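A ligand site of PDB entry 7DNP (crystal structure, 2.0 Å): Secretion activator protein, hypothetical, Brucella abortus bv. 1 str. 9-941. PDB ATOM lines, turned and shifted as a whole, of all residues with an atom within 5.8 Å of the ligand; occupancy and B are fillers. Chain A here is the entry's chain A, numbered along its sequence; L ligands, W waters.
The side-chain hydroxyl (OH) of Tyr 69 lies within hydrogen-bond range of an oxygen (O6) of the ligand (2.5 Å).
A nitrogen (N2) of the ligand is in hydrogen-bond range of the backbone carbonyl oxygen of Ile 91.
An oxygen (O8) of the ligand is in hydrogen-bond range of the backbone carbonyl oxygen (O) of Gly 34, 2.7 Å away.
An oxygen (O10) of the ligand sits at hydrogen-bond distance from the indole nitrogen of Trp 155 (2.8 Å).
The backbone carbonyl oxygen of His 92 sits at hydrogen-bond distance from a nitrogen (N3) of the ligand.
O10 of the ligand is in hydrogen-bond range of NE2 of His 92.
An oxygen (O12) of the ligand is in hydrogen-bond range of the side-chain hydroxyl (OG1) of Thr 39 (2.9 Å).
OG of Ser 93 is in hydrogen-bond range of O13 of the ligand (3.0 Å).
O12 of the ligand lies within hydrogen-bond range of N of Thr 36, 3.2 Å away.
OG1 of Thr 36 sits close to O12 of the ligand (3.4 Å).
An oxygen (O7) of the ligand sits close to the backbone NH (N) of Gly 94.
The side-chain hydroxyl (OH) of Tyr 69 lies within hydrogen-bond range of the side-chain hydroxyl (OG1) of Thr 39, 3.0 Å away.
NE1 of Trp 155 sits at hydrogen-bond distance from NE2 of His 92.
OG1 of Thr 36 is in hydrogen-bond range of N of Thr 39 (3.3 Å).
OH of Tyr 65 is in hydrogen-bond range of O of Met 33, 2.6 Å away.
CA of Gly 28 touches C17 of the ligand, at 3.9 Å.
Thr 31 touches the ligand.
Ile 35 touches the ligand.
Tyr 65 touches the ligand.
CH2 of Trp 141 touches O13 of the ligand, 3.5 Å away.
CD2 of Leu 142 touches C23 of the ligand (3.7 Å).
Leu 145 touches the ligand.
CD2 of Phe 151 touches C19 of the ligand, 3.6 Å away.
Hydrophobic or aromatic side chains that line the ligand: Ile 35, Tyr 65, Tyr 69, Ile 91, His 92, Trp 141, Leu 142, Leu 145, Phe 151 and Trp 155.
Water W1 bridges O of Pro 27 and N1 of the ligand.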
ATOM      1  N   GLU A  17      16.670 -19.995  18.590  1.00  0.00           N
ATOM      2  CA  GLU A  17      16.895 -21.307  19.194  1.00  0.00           C
ATOM      3  C   GLU A  17      18.249 -21.907  18.861  1.00  0.00           C
ATOM      4  O   GLU A  17      18.845 -22.576  19.705  1.00  0.00           O
ATOM      5  CB  GLU A  17      15.797 -22.289  18.752  1.00  0.00           C
ATOM      6  CG  GLU A  17      14.486 -22.117  19.475  1.00  0.00           C
ATOM      7  CD  GLU A  17      14.656 -22.097  20.971  1.00  0.00           C
ATOM      8  OE1 GLU A  17      15.328 -23.011  21.506  1.00  0.00           O
ATOM      9  OE2 GLU A  17      14.130 -21.161  21.610  1.00  0.00           O
ATOM     10  N   PRO A  27      17.362 -28.758  33.986  1.00  0.00           N
ATOM     11  CA  PRO A  27      16.153 -29.555  33.746  1.00  0.00           C
ATOM     12  C   PRO A  27      15.634 -29.318  32.339  1.00  0.00           C
ATOM     13  O   PRO A  27      15.904 -28.280  31.713  1.00  0.00           O
ATOM     14  CB  PRO A  27      15.166 -29.057  34.803  1.00  0.00           C
ATOM     15  CG  PRO A  27      15.655 -27.693  35.153  1.00  0.00           C
ATOM     16  CD  PRO A  27      17.158 -27.736  35.015  1.00  0.00           C
ATOM     17  N   GLY A  28      14.882 -30.300  31.830  1.00  0.00           N
ATOM     18  CA  GLY A  28      14.297 -30.241  30.507  1.00  0.00           C
ATOM     19  C   GLY A  28      14.990 -31.126  29.484  1.00  0.00           C
ATOM     20  O   GLY A  28      14.332 -31.615  28.558  1.00  0.00           O
ATOM     21  N   GLY A  29      16.301 -31.342  29.632  1.00  0.00           N
ATOM     22  CA  GLY A  29      17.005 -32.208  28.708  1.00  0.00           C
ATOM     23  C   GLY A  29      17.314 -31.524  27.385  1.00  0.00           C
ATOM     24  O   GLY A  29      17.009 -30.366  27.149  1.00  0.00           O
ATOM     25  N   THR A  31      17.693 -30.328  23.497  1.00  0.00           N
ATOM     26  CA  THR A  31      16.775 -29.820  22.501  1.00  0.00           C
ATOM     27  C   THR A  31      17.509 -29.595  21.187  1.00  0.00           C
ATOM     28  O   THR A  31      18.722 -29.377  21.154  1.00  0.00           O
ATOM     29  CB  THR A  31      16.131 -28.496  22.939  1.00  0.00           C
ATOM     30  OG1 THR A  31      17.156 -27.490  23.060  1.00  0.00           O
ATOM     31  CG2 THR A  31      15.412 -28.642  24.275  1.00  0.00           C
ATOM     32  N   MET A  33      16.641 -27.105  17.820  1.00  0.00           N
ATOM     33  CA  MET A  33      15.743 -26.059  17.339  1.00  0.00           C
ATOM     34  C   MET A  33      14.589 -25.834  18.303  1.00  0.00           C
ATOM     35  O   MET A  33      13.469 -25.519  17.904  1.00  0.00           O
ATOM     36  CB  MET A  33      15.228 -26.383  15.934  1.00  0.00           C
ATOM     37  CG  MET A  33      16.347 -26.597  14.924  1.00  0.00           C
ATOM     38  SD  MET A  33      15.811 -27.490  13.469  1.00  0.00           S
ATOM     39  CE  MET A  33      15.713 -29.157  14.112  1.00  0.00           C
ATOM     40  N   GLY A  34      14.853 -26.015  19.604  1.00  0.00           N
ATOM     41  CA  GLY A  34      13.860 -25.841  20.637  1.00  0.00           C
ATOM     42  C   GLY A  34      13.019 -27.059  20.932  1.00  0.00           C
ATOM     43  O   GLY A  34      12.259 -27.049  21.909  1.00  0.00           O
ATOM     44  N   ILE A  35      13.121 -28.124  20.138  1.00  0.00           N
ATOM     45  CA  ILE A  35      12.290 -29.308  20.299  1.00  0.00           C
ATOM     46  C   ILE A  35      12.940 -30.229  21.339  1.00  0.00           C
ATOM     47  O   ILE A  35      14.095 -30.637  21.187  1.00  0.00           O
ATOM     48  CB  ILE A  35      12.107 -30.048  18.969  1.00  0.00           C
ATOM     49  CG1 ILE A  35      11.522 -29.095  17.913  1.00  0.00           C
ATOM     50  CG2 ILE A  35      11.222 -31.276  19.144  1.00  0.00           C
ATOM     51  CD1 ILE A  35      10.076 -28.746  18.162  1.00  0.00           C
ATOM     52  N   THR A  36      12.178 -30.560  22.393  1.00  0.00           N
ATOM     53  CA  THR A  36      12.702 -31.415  23.448  1.00  0.00           C
ATOM     54  C   THR A  36      12.500 -32.889  23.094  1.00  0.00           C
ATOM     55  O   THR A  36      11.807 -33.243  22.139  1.00  0.00           O
ATOM     56  CB  THR A  36      12.011 -31.136  24.787  1.00  0.00           C
ATOM     57  OG1 THR A  36      10.674 -31.646  24.748  1.00  0.00           O
ATOM     58  CG2 THR A  36      11.992 -29.639  25.080  1.00  0.00           C
ATOM     59  N   THR A  39       8.840 -34.061  23.426  1.00  0.00           N
ATOM     60  CA  THR A  39       8.007 -33.606  22.320  1.00  0.00           C
ATOM     61  C   THR A  39       8.258 -34.433  21.061  1.00  0.00           C
ATOM     62  O   THR A  39       7.314 -34.796  20.353  1.00  0.00           O
ATOM     63  CB  THR A  39       8.249 -32.119  22.069  1.00  0.00           C
ATOM     64  OG1 THR A  39       7.766 -31.379  23.194  1.00  0.00           O
ATOM     65  CG2 THR A  39       7.526 -31.652  20.812  1.00  0.00           C
ATOM     66  N   TYR A  65       6.094 -27.826  15.268  1.00  0.00           N
ATOM     67  CA  TYR A  65       5.657 -26.503  15.699  1.00  0.00           C
ATOM     68  C   TYR A  65       4.305 -26.142  15.101  1.00  0.00           C
ATOM     69  O   TYR A  65       3.466 -25.521  15.767  1.00  0.00           O
ATOM     70  CB  TYR A  65       6.707 -25.459  15.320  1.00  0.00           C
ATOM     71  CG  TYR A  65       7.873 -25.372  16.284  1.00  0.00           C
ATOM     72  CD1 TYR A  65       7.663 -25.249  17.656  1.00  0.00           C
ATOM     73  CD2 TYR A  65       9.186 -25.436  15.835  1.00  0.00           C
ATOM     74  CE1 TYR A  65       8.725 -25.173  18.545  1.00  0.00           C
ATOM     75  CE2 TYR A  65      10.253 -25.365  16.712  1.00  0.00           C
ATOM     76  CZ  TYR A  65      10.018 -25.233  18.065  1.00  0.00           C
ATOM     77  OH  TYR A  65      11.088 -25.167  18.929  1.00  0.00           O
ATOM     78  N   TYR A  69       1.760 -27.021  18.219  1.00  0.00           N
ATOM     79  CA  TYR A  69       1.843 -25.791  18.986  1.00  0.00           C
ATOM     80  C   TYR A  69       0.926 -24.739  18.380  1.00  0.00           C
ATOM     81  O   TYR A  69      -0.069 -24.357  18.999  1.00  0.00           O
ATOM     82  CB  TYR A  69       3.300 -25.330  19.088  1.00  0.00           C
ATOM     83  CG  TYR A  69       4.109 -26.267  19.948  1.00  0.00           C
ATOM     84  CD1 TYR A  69       4.132 -26.130  21.332  1.00  0.00           C
ATOM     85  CD2 TYR A  69       4.802 -27.336  19.386  1.00  0.00           C
ATOM     86  CE1 TYR A  69       4.843 -27.007  22.132  1.00  0.00           C
ATOM     87  CE2 TYR A  69       5.523 -28.223  20.184  1.00  0.00           C
ATOM     88  CZ  TYR A  69       5.537 -28.053  21.546  1.00  0.00           C
ATOM     89  OH  TYR A  69       6.242 -28.924  22.334  1.00  0.00           O
ATOM     90  N   ALA A  90       3.124 -21.210  24.418  1.00  0.00           N
ATOM     91  CA  ALA A  90       2.896 -22.630  24.154  1.00  0.00           C
ATOM     92  C   ALA A  90       4.190 -23.373  23.901  1.00  0.00           C
ATOM     93  O   ALA A  90       4.369 -24.507  24.348  1.00  0.00           O
ATOM     94  CB  ALA A  90       1.940 -22.797  22.962  1.00  0.00           C
ATOM     95  N   ILE A  91       5.124 -22.750  23.170  1.00  0.00           N
ATOM     96  CA  ILE A  91       6.393 -23.418  22.897  1.00  0.00           C
ATOM     97  C   ILE A  91       7.172 -23.632  24.189  1.00  0.00           C
ATOM     98  O   ILE A  91       7.753 -24.696  24.413  1.00  0.00           O
ATOM     99  CB  ILE A  91       7.213 -22.608  21.874  1.00  0.00           C
ATOM    100  CG1 ILE A  91       6.576 -22.699  20.487  1.00  0.00           C
ATOM    101  CG2 ILE A  91       8.666 -23.100  21.845  1.00  0.00           C
ATOM    102  CD1 ILE A  91       7.198 -21.755  19.472  1.00  0.00           C
ATOM    103  N   HIS A  92       7.135 -22.633  25.074  1.00  0.00           N
ATOM    104  CA  HIS A  92       7.939 -22.649  26.285  1.00  0.00           C
ATOM    105  C   HIS A  92       7.340 -23.531  27.380  1.00  0.00           C
ATOM    106  O   HIS A  92       8.084 -24.167  28.125  1.00  0.00           O
ATOM    107  CB  HIS A  92       8.088 -21.213  26.802  1.00  0.00           C
ATOM    108  CG  HIS A  92       9.219 -21.013  27.760  1.00  0.00           C
ATOM    109  ND1 HIS A  92       9.151 -20.127  28.803  1.00  0.00           N
ATOM    110  CD2 HIS A  92      10.452 -21.572  27.806  1.00  0.00           C
ATOM    111  CE1 HIS A  92      10.295 -20.146  29.462  1.00  0.00           C
ATOM    112  NE2 HIS A  92      11.098 -21.013  28.883  1.00  0.00           N
ATOM    113  N   SER A  93       6.011 -23.591  27.469  1.00  0.00           N
ATOM    114  CA  SER A  93       5.348 -24.217  28.606  1.00  0.00           C
ATOM    115  C   SER A  93       4.232 -25.179  28.190  1.00  0.00           C
ATOM    116  O   SER A  93       3.520 -25.687  29.065  1.00  0.00           O
ATOM    117  CB  SER A  93       4.775 -23.152  29.545  1.00  0.00           C
ATOM    118  OG  SER A  93       5.762 -22.230  29.944  1.00  0.00           O
ATOM    119  N   GLY A  94       4.062 -25.426  26.902  1.00  0.00           N
ATOM    120  CA  GLY A  94       3.021 -26.325  26.455  1.00  0.00           C
ATOM    121  C   GLY A  94       1.752 -25.598  26.070  1.00  0.00           C
ATOM    122  O   GLY A  94       1.393 -24.579  26.668  1.00  0.00           O
ATOM    123  N   PRO A  95       1.048 -26.101  25.057  1.00  0.00           N
ATOM    124  CA  PRO A  95      -0.162 -25.416  24.580  1.00  0.00           C
ATOM    125  C   PRO A  95      -1.265 -25.334  25.613  1.00  0.00           C
ATOM    126  O   PRO A  95      -2.026 -24.357  25.615  1.00  0.00           O
ATOM    127  CB  PRO A  95      -0.598 -26.261  23.375  1.00  0.00           C
ATOM    128  CG  PRO A  95       0.582 -27.081  23.020  1.00  0.00           C
ATOM    129  CD  PRO A  95       1.340 -27.309  24.272  1.00  0.00           C
ATOM    130  N   TRP A 141       3.219 -16.318  36.504  1.00  0.00           N
ATOM    131  CA  TRP A 141       3.189 -17.763  36.663  1.00  0.00           C
ATOM    132  C   TRP A 141       4.600 -18.342  36.716  1.00  0.00           C
ATOM    133  O   TRP A 141       4.859 -19.261  37.501  1.00  0.00           O
ATOM    134  CB  TRP A 141       2.379 -18.402  35.533  1.00  0.00           C
ATOM    135  CG  TRP A 141       2.385 -19.898  35.573  1.00  0.00           C
ATOM    136  CD1 TRP A 141       1.640 -20.712  36.385  1.00  0.00           C
ATOM    137  CD2 TRP A 141       3.168 -20.769  34.754  1.00  0.00           C
ATOM    138  NE1 TRP A 141       1.922 -22.024  36.122  1.00  0.00           N
ATOM    139  CE2 TRP A 141       2.855 -22.092  35.118  1.00  0.00           C
ATOM    140  CE3 TRP A 141       4.112 -20.563  33.740  1.00  0.00           C
ATOM    141  CZ2 TRP A 141       3.459 -23.203  34.520  1.00  0.00           C
ATOM    142  CZ3 TRP A 141       4.706 -21.664  33.142  1.00  0.00           C
ATOM    143  CH2 TRP A 141       4.367 -22.966  33.530  1.00  0.00           C
ATOM    144  N   LEU A 142       5.518 -17.831  35.895  1.00  0.00           N
ATOM    145  CA  LEU A 142       6.881 -18.334  35.905  1.00  0.00           C
ATOM    146  C   LEU A 142       7.567 -18.095  37.245  1.00  0.00           C
ATOM    147  O   LEU A 142       8.388 -18.917  37.675  1.00  0.00           O
ATOM    148  CB  LEU A 142       7.692 -17.706  34.773  1.00  0.00           C
ATOM    149  CG  LEU A 142       7.303 -18.095  33.353  1.00  0.00           C
ATOM    150  CD1 LEU A 142       7.948 -17.167  32.327  1.00  0.00           C
ATOM    151  CD2 LEU A 142       7.660 -19.547  33.062  1.00  0.00           C
ATOM    152  N   LEU A 145       7.597 -20.937  39.824  1.00  0.00           N
ATOM    153  CA  LEU A 145       8.329 -22.170  39.592  1.00  0.00           C
ATOM    154  C   LEU A 145       9.660 -22.158  40.337  1.00  0.00           C
ATOM    155  O   LEU A 145      10.319 -21.117  40.474  1.00  0.00           O
ATOM    156  CB  LEU A 145       8.588 -22.383  38.111  1.00  0.00           C
ATOM    157  CG  LEU A 145       7.365 -22.400  37.183  1.00  0.00           C
ATOM    158  CD1 LEU A 145       7.805 -22.475  35.731  1.00  0.00           C
ATOM    159  CD2 LEU A 145       6.438 -23.550  37.536  1.00  0.00           C
ATOM    160  N   THR A 147      12.343 -23.338  39.247  1.00  0.00           N
ATOM    161  CA  THR A 147      13.392 -23.057  38.269  1.00  0.00           C
ATOM    162  C   THR A 147      13.574 -21.575  38.002  1.00  0.00           C
ATOM    163  O   THR A 147      14.534 -21.214  37.304  1.00  0.00           O
ATOM    164  CB  THR A 147      13.097 -23.779  36.959  1.00  0.00           C
ATOM    165  OG1 THR A 147      11.704 -23.642  36.651  1.00  0.00           O
ATOM    166  CG2 THR A 147      13.451 -25.255  37.053  1.00  0.00           C
ATOM    167  N   PHE A 151      16.549 -19.626  35.841  1.00  0.00           N
ATOM    168  CA  PHE A 151      16.261 -19.169  34.478  1.00  0.00           C
ATOM    169  C   PHE A 151      15.438 -17.892  34.415  1.00  0.00           C
ATOM    170  O   PHE A 151      15.140 -17.432  33.316  1.00  0.00           O
ATOM    171  CB  PHE A 151      15.550 -20.288  33.712  1.00  0.00           C
ATOM    172  CG  PHE A 151      16.302 -21.593  33.693  1.00  0.00           C
ATOM    173  CD1 PHE A 151      17.427 -21.747  32.898  1.00  0.00           C
ATOM    174  CD2 PHE A 151      15.893 -22.645  34.492  1.00  0.00           C
ATOM    175  CE1 PHE A 151      18.133 -22.952  32.898  1.00  0.00           C
ATOM    176  CE2 PHE A 151      16.599 -23.841  34.498  1.00  0.00           C
ATOM    177  CZ  PHE A 151      17.714 -23.994  33.699  1.00  0.00           C
ATOM    178  N   TRP A 155      14.289 -15.807  31.187  1.00  0.00           N
ATOM    179  CA  TRP A 155      12.854 -15.885  30.881  1.00  0.00           C
ATOM    180  C   TRP A 155      12.241 -14.496  30.787  1.00  0.00           C
ATOM    181  O   TRP A 155      11.436 -14.231  29.884  1.00  0.00           O
ATOM    182  CB  TRP A 155      12.141 -16.697  31.962  1.00  0.00           C
ATOM    183  CG  TRP A 155      12.346 -18.181  31.902  1.00  0.00           C
ATOM    184  CD1 TRP A 155      12.911 -18.895  30.887  1.00  0.00           C
ATOM    185  CD2 TRP A 155      11.975 -19.140  32.899  1.00  0.00           C
ATOM    186  NE1 TRP A 155      12.919 -20.232  31.191  1.00  0.00           N
ATOM    187  CE2 TRP A 155      12.351 -20.409  32.421  1.00  0.00           C
ATOM    188  CE3 TRP A 155      11.362 -19.041  34.155  1.00  0.00           C
ATOM    189  CZ2 TRP A 155      12.134 -21.575  33.149  1.00  0.00           C
ATOM    190  CZ3 TRP A 155      11.158 -20.204  34.878  1.00  0.00           C
ATOM    191  CH2 TRP A 155      11.535 -21.449  34.377  1.00  0.00           C
ATOM    192  N   ARG A 158      13.098 -13.035  27.522  1.00  0.00           N
ATOM    193  CA  ARG A 158      12.360 -13.690  26.451  1.00  0.00           C
ATOM    194  C   ARG A 158      10.934 -13.131  26.346  1.00  0.00           C
ATOM    195  O   ARG A 158      10.460 -12.836  25.253  1.00  0.00           O
ATOM    196  CB  ARG A 158      12.326 -15.196  26.686  1.00  0.00           C
ATOM    197  CG  ARG A 158      11.351 -15.946  25.789  1.00  0.00           C
ATOM    198  CD  ARG A 158      11.436 -17.444  25.995  1.00  0.00           C
ATOM    199  NE  ARG A 158      10.651 -18.172  24.999  1.00  0.00           N
ATOM    200  CZ  ARG A 158      10.877 -19.429  24.643  1.00  0.00           C
ATOM    201  NH1 ARG A 158      11.880 -20.111  25.188  1.00  0.00           N
ATOM    202  NH2 ARG A 158      10.105 -20.016  23.726  1.00  0.00           N
HETATM  203  C1  LIG L   1      11.191 -25.792  26.544  1.00  0.00           C
HETATM  204  C2  LIG L   1      12.872 -24.685  27.945  1.00  0.00           C
HETATM  205  C3  LIG L   1      12.033 -25.435  25.310  1.00  0.00           C
HETATM  206  C4  LIG L   1      13.750 -24.451  26.712  1.00  0.00           C
HETATM  207  C5  LIG L   1      12.010 -25.874  27.777  1.00  0.00           C
HETATM  208  C6  LIG L   1       9.174 -27.029  26.522  1.00  0.00           C
HETATM  209  C7  LIG L   1       8.434 -27.892  25.464  1.00  0.00           C
HETATM  210  C8  LIG L   1       6.988 -27.987  25.773  1.00  0.00           C
HETATM  211  C9  LIG L   1       6.737 -28.427  27.151  1.00  0.00           C
HETATM  212  C10 LIG L   1       7.430 -27.483  28.133  1.00  0.00           C
HETATM  213  C11 LIG L   1      11.474 -26.566  30.107  1.00  0.00           C
HETATM  214  C12 LIG L   1      11.140 -25.052  24.164  1.00  0.00           C
HETATM  215  C13 LIG L   1       7.138 -27.870  29.556  1.00  0.00           C
HETATM  216  C14 LIG L   1      13.807 -23.736  30.098  1.00  0.00           C
HETATM  217  C15 LIG L   1      10.801 -25.768  31.214  1.00  0.00           C
HETATM  218  C16 LIG L   1       9.095 -27.897  22.926  1.00  0.00           C
HETATM  219  C17 LIG L   1      11.057 -28.033  30.170  1.00  0.00           C
HETATM  220  C18 LIG L   1       9.235 -23.894  31.870  1.00  0.00           C
HETATM  221  C19 LIG L   1      14.732 -23.823  31.302  1.00  0.00           C
HETATM  222  C20 LIG L   1       9.155 -27.082  21.635  1.00  0.00           C
HETATM  223  C21 LIG L   1       7.967 -24.656  32.251  1.00  0.00           C
HETATM  224  C22 LIG L   1       6.868 -26.451  33.682  1.00  0.00           C
HETATM  225  C23 LIG L   1       8.858 -22.527  31.324  1.00  0.00           C
HETATM  226  C24 LIG L   1       6.885 -27.786  32.953  1.00  0.00           C
HETATM  227  C25 LIG L   1       6.910 -26.726  35.175  1.00  0.00           C
HETATM  228  C26 LIG L   1       5.500 -26.893  35.741  1.00  0.00           C
HETATM  229  C27 LIG L   1       5.531 -27.121  37.254  1.00  0.00           C
HETATM  230  N1  LIG L   1      13.779 -24.796  29.129  1.00  0.00           N
HETATM  231  N2  LIG L   1       8.574 -27.248  24.120  1.00  0.00           N
HETATM  232  N3  LIG L   1       9.893 -24.674  30.838  1.00  0.00           N
HETATM  233  N4  LIG L   1       8.044 -25.685  33.287  1.00  0.00           N
HETATM  234  O1  LIG L   1      10.538 -27.070  26.324  1.00  0.00           O
HETATM  235  O2  LIG L   1      12.937 -24.298  25.518  1.00  0.00           O
HETATM  236  O3  LIG L   1       8.873 -27.484  27.882  1.00  0.00           O
HETATM  237  O4  LIG L   1      11.039 -25.980  28.903  1.00  0.00           O
HETATM  238  O5  LIG L   1      14.591 -25.520  26.540  1.00  0.00           O
HETATM  239  O6  LIG L   1       6.319 -28.912  24.823  1.00  0.00           O
HETATM  240  O7  LIG L   1       5.322 -28.430  27.412  1.00  0.00           O
HETATM  241  O8  LIG L   1      11.967 -24.613  23.122  1.00  0.00           O
HETATM  242  O9  LIG L   1       7.628 -29.165  29.790  1.00  0.00           O
HETATM  243  O10 LIG L   1      13.114 -22.777  29.964  1.00  0.00           O
HETATM  244  O11 LIG L   1      11.006 -26.018  32.357  1.00  0.00           O
HETATM  245  O12 LIG L   1       9.455 -29.038  22.930  1.00  0.00           O
HETATM  246  O13 LIG L   1       6.953 -24.409  31.682  1.00  0.00           O
HETATM  247  O14 LIG L   1       5.802 -28.317  32.592  1.00  0.00           O
HETATM  248  O15 LIG L   1       7.984 -28.355  32.717  1.00  0.00           O
HETATM  249  O16 LIG L   1       6.642 -27.125  37.858  1.00  0.00           O
HETATM  250  O17 LIG L   1       4.459 -27.299  37.889  1.00  0.00           O
HETATM  251  O   HOH W   1      15.749 -26.566  29.861  1.00  0.00           O
HETATM  252  O   HOH W   2       3.809 -29.710  25.005  1.00  0.00           O
HETATM  253  O   HOH W   3       7.637 -25.756  40.338  1.00  0.00           O
